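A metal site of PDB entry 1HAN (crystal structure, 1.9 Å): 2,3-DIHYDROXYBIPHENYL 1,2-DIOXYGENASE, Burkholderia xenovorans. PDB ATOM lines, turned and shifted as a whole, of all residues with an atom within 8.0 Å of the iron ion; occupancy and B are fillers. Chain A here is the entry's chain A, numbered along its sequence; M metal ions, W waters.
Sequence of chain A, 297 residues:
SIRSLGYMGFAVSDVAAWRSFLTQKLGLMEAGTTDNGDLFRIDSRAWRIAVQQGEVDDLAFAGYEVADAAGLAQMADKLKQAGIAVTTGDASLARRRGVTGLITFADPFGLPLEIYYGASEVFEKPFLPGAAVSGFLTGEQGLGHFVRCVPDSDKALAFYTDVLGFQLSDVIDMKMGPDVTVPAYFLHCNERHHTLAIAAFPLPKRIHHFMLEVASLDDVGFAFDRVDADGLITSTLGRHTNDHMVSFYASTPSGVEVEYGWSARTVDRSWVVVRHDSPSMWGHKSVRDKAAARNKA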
ATOM      1  N   GLY A 144     -32.016  29.152 -26.775  1.00  0.00           N
ATOM      2  CA  GLY A 144     -31.088  28.306 -27.485  1.00  0.00           C
ATOM      3  C   GLY A 144     -31.927  27.218 -28.121  1.00  0.00           C
ATOM      4  O   GLY A 144     -32.987  27.523 -28.667  1.00  0.00           O
ATOM      5  N   HIS A 145     -31.503  25.958 -28.020  1.00  0.00           N
ATOM      6  CA  HIS A 145     -32.302  24.874 -28.578  1.00  0.00           C
ATOM      7  C   HIS A 145     -32.098  23.553 -27.849  1.00  0.00           C
ATOM      8  O   HIS A 145     -31.238  23.450 -26.963  1.00  0.00           O
ATOM      9  CB  HIS A 145     -32.018  24.675 -30.086  1.00  0.00           C
ATOM     10  CG  HIS A 145     -30.638  24.199 -30.424  1.00  0.00           C
ATOM     11  ND1 HIS A 145     -29.838  24.779 -31.379  1.00  0.00           N
ATOM     12  CD2 HIS A 145     -29.954  23.101 -29.989  1.00  0.00           C
ATOM     13  CE1 HIS A 145     -28.715  24.055 -31.511  1.00  0.00           C
ATOM     14  NE2 HIS A 145     -28.721  23.018 -30.690  1.00  0.00           N
ATOM     15  N   PHE A 146     -32.939  22.575 -28.130  1.00  0.00           N
ATOM     16  CA  PHE A 146     -32.775  21.245 -27.547  1.00  0.00           C
ATOM     17  C   PHE A 146     -33.299  20.229 -28.544  1.00  0.00           C
ATOM     18  O   PHE A 146     -34.073  20.570 -29.445  1.00  0.00           O
ATOM     19  CB  PHE A 146     -33.387  21.095 -26.139  1.00  0.00           C
ATOM     20  CG  PHE A 146     -34.886  21.233 -26.060  1.00  0.00           C
ATOM     21  CD1 PHE A 146     -35.734  20.253 -26.583  1.00  0.00           C
ATOM     22  CD2 PHE A 146     -35.451  22.313 -25.377  1.00  0.00           C
ATOM     23  CE1 PHE A 146     -37.123  20.346 -26.436  1.00  0.00           C
ATOM     24  CE2 PHE A 146     -36.846  22.423 -25.222  1.00  0.00           C
ATOM     25  CZ  PHE A 146     -37.678  21.429 -25.751  1.00  0.00           C
ATOM     26  N   VAL A 147     -32.764  19.027 -28.450  1.00  0.00           N
ATOM     27  CA  VAL A 147     -33.139  17.925 -29.332  1.00  0.00           C
ATOM     28  C   VAL A 147     -34.024  16.988 -28.534  1.00  0.00           C
ATOM     29  O   VAL A 147     -33.597  16.429 -27.523  1.00  0.00           O
ATOM     30  CB  VAL A 147     -31.889  17.175 -29.846  1.00  0.00           C
ATOM     31  CG1 VAL A 147     -32.303  16.020 -30.772  1.00  0.00           C
ATOM     32  CG2 VAL A 147     -30.952  18.144 -30.563  1.00  0.00           C
ATOM     33  N   PHE A 186     -34.546  19.333 -37.973  1.00  0.00           N
ATOM     34  CA  PHE A 186     -34.238  20.602 -37.291  1.00  0.00           C
ATOM     35  C   PHE A 186     -35.264  21.648 -37.673  1.00  0.00           C
ATOM     36  O   PHE A 186     -35.462  21.946 -38.865  1.00  0.00           O
ATOM     37  CB  PHE A 186     -32.806  21.020 -37.639  1.00  0.00           C
ATOM     38  CG  PHE A 186     -31.784  20.003 -37.222  1.00  0.00           C
ATOM     39  CD1 PHE A 186     -31.546  18.869 -38.017  1.00  0.00           C
ATOM     40  CD2 PHE A 186     -31.127  20.114 -36.001  1.00  0.00           C
ATOM     41  CE1 PHE A 186     -30.686  17.854 -37.589  1.00  0.00           C
ATOM     42  CE2 PHE A 186     -30.252  19.105 -35.548  1.00  0.00           C
ATOM     43  CZ  PHE A 186     -30.036  17.978 -36.352  1.00  0.00           C
ATOM     44  N   HIS A 194     -32.093  26.444 -35.482  1.00  0.00           N
ATOM     45  CA  HIS A 194     -33.115  25.586 -34.934  1.00  0.00           C
ATOM     46  C   HIS A 194     -33.280  25.858 -33.459  1.00  0.00           C
ATOM     47  O   HIS A 194     -32.317  26.181 -32.767  1.00  0.00           O
ATOM     48  CB  HIS A 194     -32.914  24.082 -35.237  1.00  0.00           C
ATOM     49  CG  HIS A 194     -31.692  23.471 -34.618  1.00  0.00           C
ATOM     50  ND1 HIS A 194     -30.442  23.567 -35.185  1.00  0.00           N
ATOM     51  CD2 HIS A 194     -31.553  22.653 -33.536  1.00  0.00           C
ATOM     52  CE1 HIS A 194     -29.589  22.822 -34.506  1.00  0.00           C
ATOM     53  NE2 HIS A 194     -30.235  22.265 -33.496  1.00  0.00           N
ATOM     54  N   ALA A 197     -35.169  20.262 -32.393  1.00  0.00           N
ATOM     55  CA  ALA A 197     -34.807  19.207 -33.339  1.00  0.00           C
ATOM     56  C   ALA A 197     -35.548  17.944 -32.806  1.00  0.00           C
ATOM     57  O   ALA A 197     -35.814  17.831 -31.599  1.00  0.00           O
ATOM     58  CB  ALA A 197     -33.307  18.991 -33.398  1.00  0.00           C
ATOM     59  N   HIS A 208     -31.703  14.831 -26.125  1.00  0.00           N
ATOM     60  CA  HIS A 208     -30.331  14.419 -26.326  1.00  0.00           C
ATOM     61  C   HIS A 208     -29.447  15.510 -25.710  1.00  0.00           C
ATOM     62  O   HIS A 208     -28.491  15.213 -24.986  1.00  0.00           O
ATOM     63  CB  HIS A 208     -30.023  14.270 -27.823  1.00  0.00           C
ATOM     64  CG  HIS A 208     -28.569  14.140 -28.117  1.00  0.00           C
ATOM     65  ND1 HIS A 208     -27.837  15.133 -28.726  1.00  0.00           N
ATOM     66  CD2 HIS A 208     -27.678  13.165 -27.780  1.00  0.00           C
ATOM     67  CE1 HIS A 208     -26.559  14.798 -28.739  1.00  0.00           C
ATOM     68  NE2 HIS A 208     -26.438  13.609 -28.171  1.00  0.00           N
ATOM     69  N   HIS A 209     -29.727  16.772 -26.006  1.00  0.00           N
ATOM     70  CA  HIS A 209     -28.935  17.874 -25.441  1.00  0.00           C
ATOM     71  C   HIS A 209     -29.702  19.176 -25.545  1.00  0.00           C
ATOM     72  O   HIS A 209     -30.727  19.239 -26.220  1.00  0.00           O
ATOM     73  CB  HIS A 209     -27.586  18.040 -26.184  1.00  0.00           C
ATOM     74  CG  HIS A 209     -27.713  18.652 -27.554  1.00  0.00           C
ATOM     75  ND1 HIS A 209     -27.917  17.936 -28.713  1.00  0.00           N
ATOM     76  CD2 HIS A 209     -27.597  19.951 -27.953  1.00  0.00           C
ATOM     77  CE1 HIS A 209     -27.912  18.778 -29.751  1.00  0.00           C
ATOM     78  NE2 HIS A 209     -27.724  20.021 -29.354  1.00  0.00           N
ATOM     79  N   PHE A 210     -29.241  20.173 -24.798  1.00  0.00           N
ATOM     80  CA  PHE A 210     -29.785  21.529 -24.878  1.00  0.00           C
ATOM     81  C   PHE A 210     -28.527  22.341 -25.194  1.00  0.00           C
ATOM     82  O   PHE A 210     -27.412  21.908 -24.891  1.00  0.00           O
ATOM     83  CB  PHE A 210     -30.523  21.991 -23.604  1.00  0.00           C
ATOM     84  CG  PHE A 210     -29.658  22.149 -22.385  1.00  0.00           C
ATOM     85  CD1 PHE A 210     -29.337  21.029 -21.589  1.00  0.00           C
ATOM     86  CD2 PHE A 210     -29.211  23.407 -21.981  1.00  0.00           C
ATOM     87  CE1 PHE A 210     -28.592  21.183 -20.415  1.00  0.00           C
ATOM     88  CE2 PHE A 210     -28.475  23.562 -20.817  1.00  0.00           C
ATOM     89  CZ  PHE A 210     -28.158  22.455 -20.027  1.00  0.00           C
ATOM     90  N   MET A 211     -28.688  23.484 -25.826  1.00  0.00           N
ATOM     91  CA  MET A 211     -27.533  24.262 -26.234  1.00  0.00           C
ATOM     92  C   MET A 211     -27.627  25.686 -25.759  1.00  0.00           C
ATOM     93  O   MET A 211     -28.716  26.242 -25.636  1.00  0.00           O
ATOM     94  CB  MET A 211     -27.466  24.223 -27.771  1.00  0.00           C
ATOM     95  CG  MET A 211     -26.366  25.030 -28.450  1.00  0.00           C
ATOM     96  SD  MET A 211     -26.679  26.803 -28.488  1.00  0.00           S
ATOM     97  CE  MET A 211     -28.091  26.923 -29.553  1.00  0.00           C
ATOM     98  N   LEU A 212     -26.469  26.247 -25.410  1.00  0.00           N
ATOM     99  CA  LEU A 212     -26.357  27.651 -24.997  1.00  0.00           C
ATOM    100  C   LEU A 212     -25.298  28.210 -25.939  1.00  0.00           C
ATOM    101  O   LEU A 212     -24.291  27.551 -26.217  1.00  0.00           O
ATOM    102  CB  LEU A 212     -25.899  27.778 -23.541  1.00  0.00           C
ATOM    103  CG  LEU A 212     -26.892  27.315 -22.468  1.00  0.00           C
ATOM    104  CD1 LEU A 212     -26.213  27.366 -21.121  1.00  0.00           C
ATOM    105  CD2 LEU A 212     -28.140  28.192 -22.478  1.00  0.00           C
ATOM    106  N   HIS A 240     -20.745  21.973 -36.674  1.00  0.00           N
ATOM    107  CA  HIS A 240     -21.863  21.245 -37.293  1.00  0.00           C
ATOM    108  C   HIS A 240     -22.083  21.659 -38.740  1.00  0.00           C
ATOM    109  O   HIS A 240     -21.852  22.821 -39.122  1.00  0.00           O
ATOM    110  CB  HIS A 240     -23.161  21.427 -36.505  1.00  0.00           C
ATOM    111  CG  HIS A 240     -23.189  20.647 -35.232  1.00  0.00           C
ATOM    112  ND1 HIS A 240     -23.084  19.259 -35.200  1.00  0.00           N
ATOM    113  CD2 HIS A 240     -23.299  21.034 -33.946  1.00  0.00           C
ATOM    114  CE1 HIS A 240     -23.134  18.850 -33.949  1.00  0.00           C
ATOM    115  NE2 HIS A 240     -23.260  19.905 -33.166  1.00  0.00           N
ATOM    116  N   ASN A 242     -25.038  21.724 -40.380  1.00  0.00           N
ATOM    117  CA  ASN A 242     -26.246  22.471 -40.665  1.00  0.00           C
ATOM    118  C   ASN A 242     -26.360  23.869 -40.070  1.00  0.00           C
ATOM    119  O   ASN A 242     -26.593  24.831 -40.826  1.00  0.00           O
ATOM    120  CB  ASN A 242     -27.503  21.617 -40.412  1.00  0.00           C
ATOM    121  CG  ASN A 242     -27.659  21.185 -38.963  1.00  0.00           C
ATOM    122  OD1 ASN A 242     -26.702  21.185 -38.174  1.00  0.00           O
ATOM    123  ND2 ASN A 242     -28.883  20.805 -38.598  1.00  0.00           N
ATOM    124  N   ASP A 243     -26.160  24.008 -38.762  1.00  0.00           N
ATOM    125  CA  ASP A 243     -26.223  25.334 -38.144  1.00  0.00           C
ATOM    126  C   ASP A 243     -24.849  26.017 -38.090  1.00  0.00           C
ATOM    127  O   ASP A 243     -24.761  27.197 -37.744  1.00  0.00           O
ATOM    128  CB  ASP A 243     -26.922  25.304 -36.770  1.00  0.00           C
ATOM    129  CG  ASP A 243     -26.148  24.526 -35.691  1.00  0.00           C
ATOM    130  OD1 ASP A 243     -25.064  23.949 -35.954  1.00  0.00           O
ATOM    131  OD2 ASP A 243     -26.680  24.483 -34.563  1.00  0.00           O
ATOM    132  N   MET A 245     -22.530  25.706 -36.057  1.00  0.00           N
ATOM    133  CA  MET A 245     -22.134  26.033 -34.687  1.00  0.00           C
ATOM    134  C   MET A 245     -20.795  25.357 -34.370  1.00  0.00           C
ATOM    135  O   MET A 245     -20.589  24.180 -34.704  1.00  0.00           O
ATOM    136  CB  MET A 245     -23.191  25.490 -33.727  1.00  0.00           C
ATOM    137  CG  MET A 245     -22.928  25.709 -32.230  1.00  0.00           C
ATOM    138  SD  MET A 245     -23.758  27.160 -31.570  1.00  0.00           S
ATOM    139  CE  MET A 245     -25.450  26.689 -31.804  1.00  0.00           C
ATOM    140  N   SER A 247     -18.758  24.045 -31.446  1.00  0.00           N
ATOM    141  CA  SER A 247     -19.111  23.697 -30.071  1.00  0.00           C
ATOM    142  C   SER A 247     -18.469  22.436 -29.566  1.00  0.00           C
ATOM    143  O   SER A 247     -17.808  21.710 -30.311  1.00  0.00           O
ATOM    144  CB  SER A 247     -20.625  23.438 -30.025  1.00  0.00           C
ATOM    145  OG  SER A 247     -20.998  22.352 -30.888  1.00  0.00           O
ATOM    146  N   TYR A 249     -19.477  19.216 -26.486  1.00  0.00           N
ATOM    147  CA  TYR A 249     -20.596  18.683 -25.708  1.00  0.00           C
ATOM    148  C   TYR A 249     -20.031  18.180 -24.387  1.00  0.00           C
ATOM    149  O   TYR A 249     -18.867  17.761 -24.307  1.00  0.00           O
ATOM    150  CB  TYR A 249     -21.285  17.531 -26.437  1.00  0.00           C
ATOM    151  CG  TYR A 249     -22.115  17.942 -27.624  1.00  0.00           C
ATOM    152  CD1 TYR A 249     -21.517  18.420 -28.789  1.00  0.00           C
ATOM    153  CD2 TYR A 249     -23.498  17.811 -27.598  1.00  0.00           C
ATOM    154  CE1 TYR A 249     -22.274  18.769 -29.905  1.00  0.00           C
ATOM    155  CE2 TYR A 249     -24.265  18.149 -28.696  1.00  0.00           C
ATOM    156  CZ  TYR A 249     -23.648  18.630 -29.849  1.00  0.00           C
ATOM    157  OH  TYR A 249     -24.437  18.966 -30.938  1.00  0.00           O
ATOM    158  N   VAL A 258     -25.041  18.865 -22.610  1.00  0.00           N
ATOM    159  CA  VAL A 258     -25.188  20.277 -22.916  1.00  0.00           C
ATOM    160  C   VAL A 258     -24.182  20.582 -24.014  1.00  0.00           C
ATOM    161  O   VAL A 258     -23.072  20.012 -24.034  1.00  0.00           O
ATOM    162  CB  VAL A 258     -24.930  21.197 -21.700  1.00  0.00           C
ATOM    163  CG1 VAL A 258     -23.534  20.993 -21.142  1.00  0.00           C
ATOM    164  CG2 VAL A 258     -25.127  22.671 -22.088  1.00  0.00           C
ATOM    165  N   GLU A 259     -24.604  21.395 -24.968  1.00  0.00           N
ATOM    166  CA  GLU A 259     -23.753  21.812 -26.061  1.00  0.00           C
ATOM    167  C   GLU A 259     -23.489  23.297 -25.776  1.00  0.00           C
ATOM    168  O   GLU A 259     -24.412  24.045 -25.470  1.00  0.00           O
ATOM    169  CB  GLU A 259     -24.477  21.667 -27.395  1.00  0.00           C
ATOM    170  CG  GLU A 259     -23.652  22.169 -28.570  1.00  0.00           C
ATOM    171  CD  GLU A 259     -24.411  22.184 -29.877  1.00  0.00           C
ATOM    172  OE1 GLU A 259     -25.643  21.934 -29.893  1.00  0.00           O
ATOM    173  OE2 GLU A 259     -23.763  22.415 -30.911  1.00  0.00           O
ATOM    174  N   TYR A 260     -22.226  23.691 -25.850  1.00  0.00           N
ATOM    175  CA  TYR A 260     -21.799  25.066 -25.570  1.00  0.00           C
ATOM    176  C   TYR A 260     -21.117  25.538 -26.857  1.00  0.00           C
ATOM    177  O   TYR A 260     -20.004  25.121 -27.170  1.00  0.00           O
ATOM    178  CB  TYR A 260     -20.813  25.003 -24.403  1.00  0.00           C
ATOM    179  CG  TYR A 260     -20.642  26.288 -23.617  1.00  0.00           C
ATOM    180  CD1 TYR A 260     -21.563  26.663 -22.645  1.00  0.00           C
ATOM    181  CD2 TYR A 260     -19.502  27.073 -23.792  1.00  0.00           C
ATOM    182  CE1 TYR A 260     -21.342  27.782 -21.833  1.00  0.00           C
ATOM    183  CE2 TYR A 260     -19.269  28.191 -22.992  1.00  0.00           C
ATOM    184  CZ  TYR A 260     -20.192  28.537 -22.010  1.00  0.00           C
ATOM    185  OH  TYR A 260     -19.911  29.584 -21.165  1.00  0.00           O
ATOM    186  N   HIS A 284     -15.693  17.319 -33.196  1.00  0.00           N
ATOM    187  CA  HIS A 284     -16.788  16.610 -32.550  1.00  0.00           C
ATOM    188  C   HIS A 284     -16.490  15.110 -32.435  1.00  0.00           C
ATOM    189  O   HIS A 284     -17.350  14.270 -32.678  1.00  0.00           O
ATOM    190  CB  HIS A 284     -18.104  16.841 -33.282  1.00  0.00           C
ATOM    191  CG  HIS A 284     -18.707  18.193 -33.014  1.00  0.00           C
ATOM    192  ND1 HIS A 284     -19.459  18.868 -33.942  1.00  0.00           N
ATOM    193  CD2 HIS A 284     -18.693  18.964 -31.909  1.00  0.00           C
ATOM    194  CE1 HIS A 284     -19.891  20.001 -33.421  1.00  0.00           C
ATOM    195  NE2 HIS A 284     -19.439  20.082 -32.182  1.00  0.00           N
HETATM  196 FE    FE M   1     -27.226  21.506 -30.971  1.00  0.00          FE
HETATM  197  O   HOH W   1     -28.385  20.546 -32.469  1.00  0.00           O
HETATM  198  O   HOH W   2     -25.986  22.693 -32.652  1.00  0.00           O
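OH of Tyr 249 sits close to OE1 of Glu 259, 3.4 Å away. NE2 of His 240 sits close to OE2 of Glu 259 (3.4 Å). The backbone carbonyl oxygen of Phe 210 sits at hydrogen-bond distance from the backbone NH of Glu 259, 2.9 Å away. OE2 of Glu 259 sits at hydrogen-bond distance from OG of Ser 247, at 2.8 Å. ND1 of His 145 lies close to O of His 194 (3.2 Å). The backbone carbonyl oxygen (O) of His 145 sits at hydrogen-bond distance from the backbone NH (N) of Met 211. O of His 209 lies within hydrogen-bond range of N of Val 147 (3.0 Å). A ring nitrogen (ND1) of His 209 sits at hydrogen-bond distance from a ring nitrogen (ND1) of His 208 (2.8 Å).
Merely in contact with the iron ion: Tyr 249 (3.8 Å). Of the 22 residues printed, 4 come within 4 Å of the iron ion. Along chain A the residues within 4 Å of the iron ion span positions 145 to 259.
The side-chain carboxylate (OE1) of Glu 259 is bound to the iron ion, at 2.0 Å. Water W1 binds the iron ion (2.1 Å). The iron ion is bound by a ring nitrogen (NE2) of His 145. The iron ion is bound by NE2 of His 209, at 2.3 Å. Water W2 is bound to the iron ion.
Water W2 bridges the side-chain carboxylate (OD2) of Asp 243 (2.7 Å) and the side-chain carboxylate (OE2) of Glu 259 (2.8 Å).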
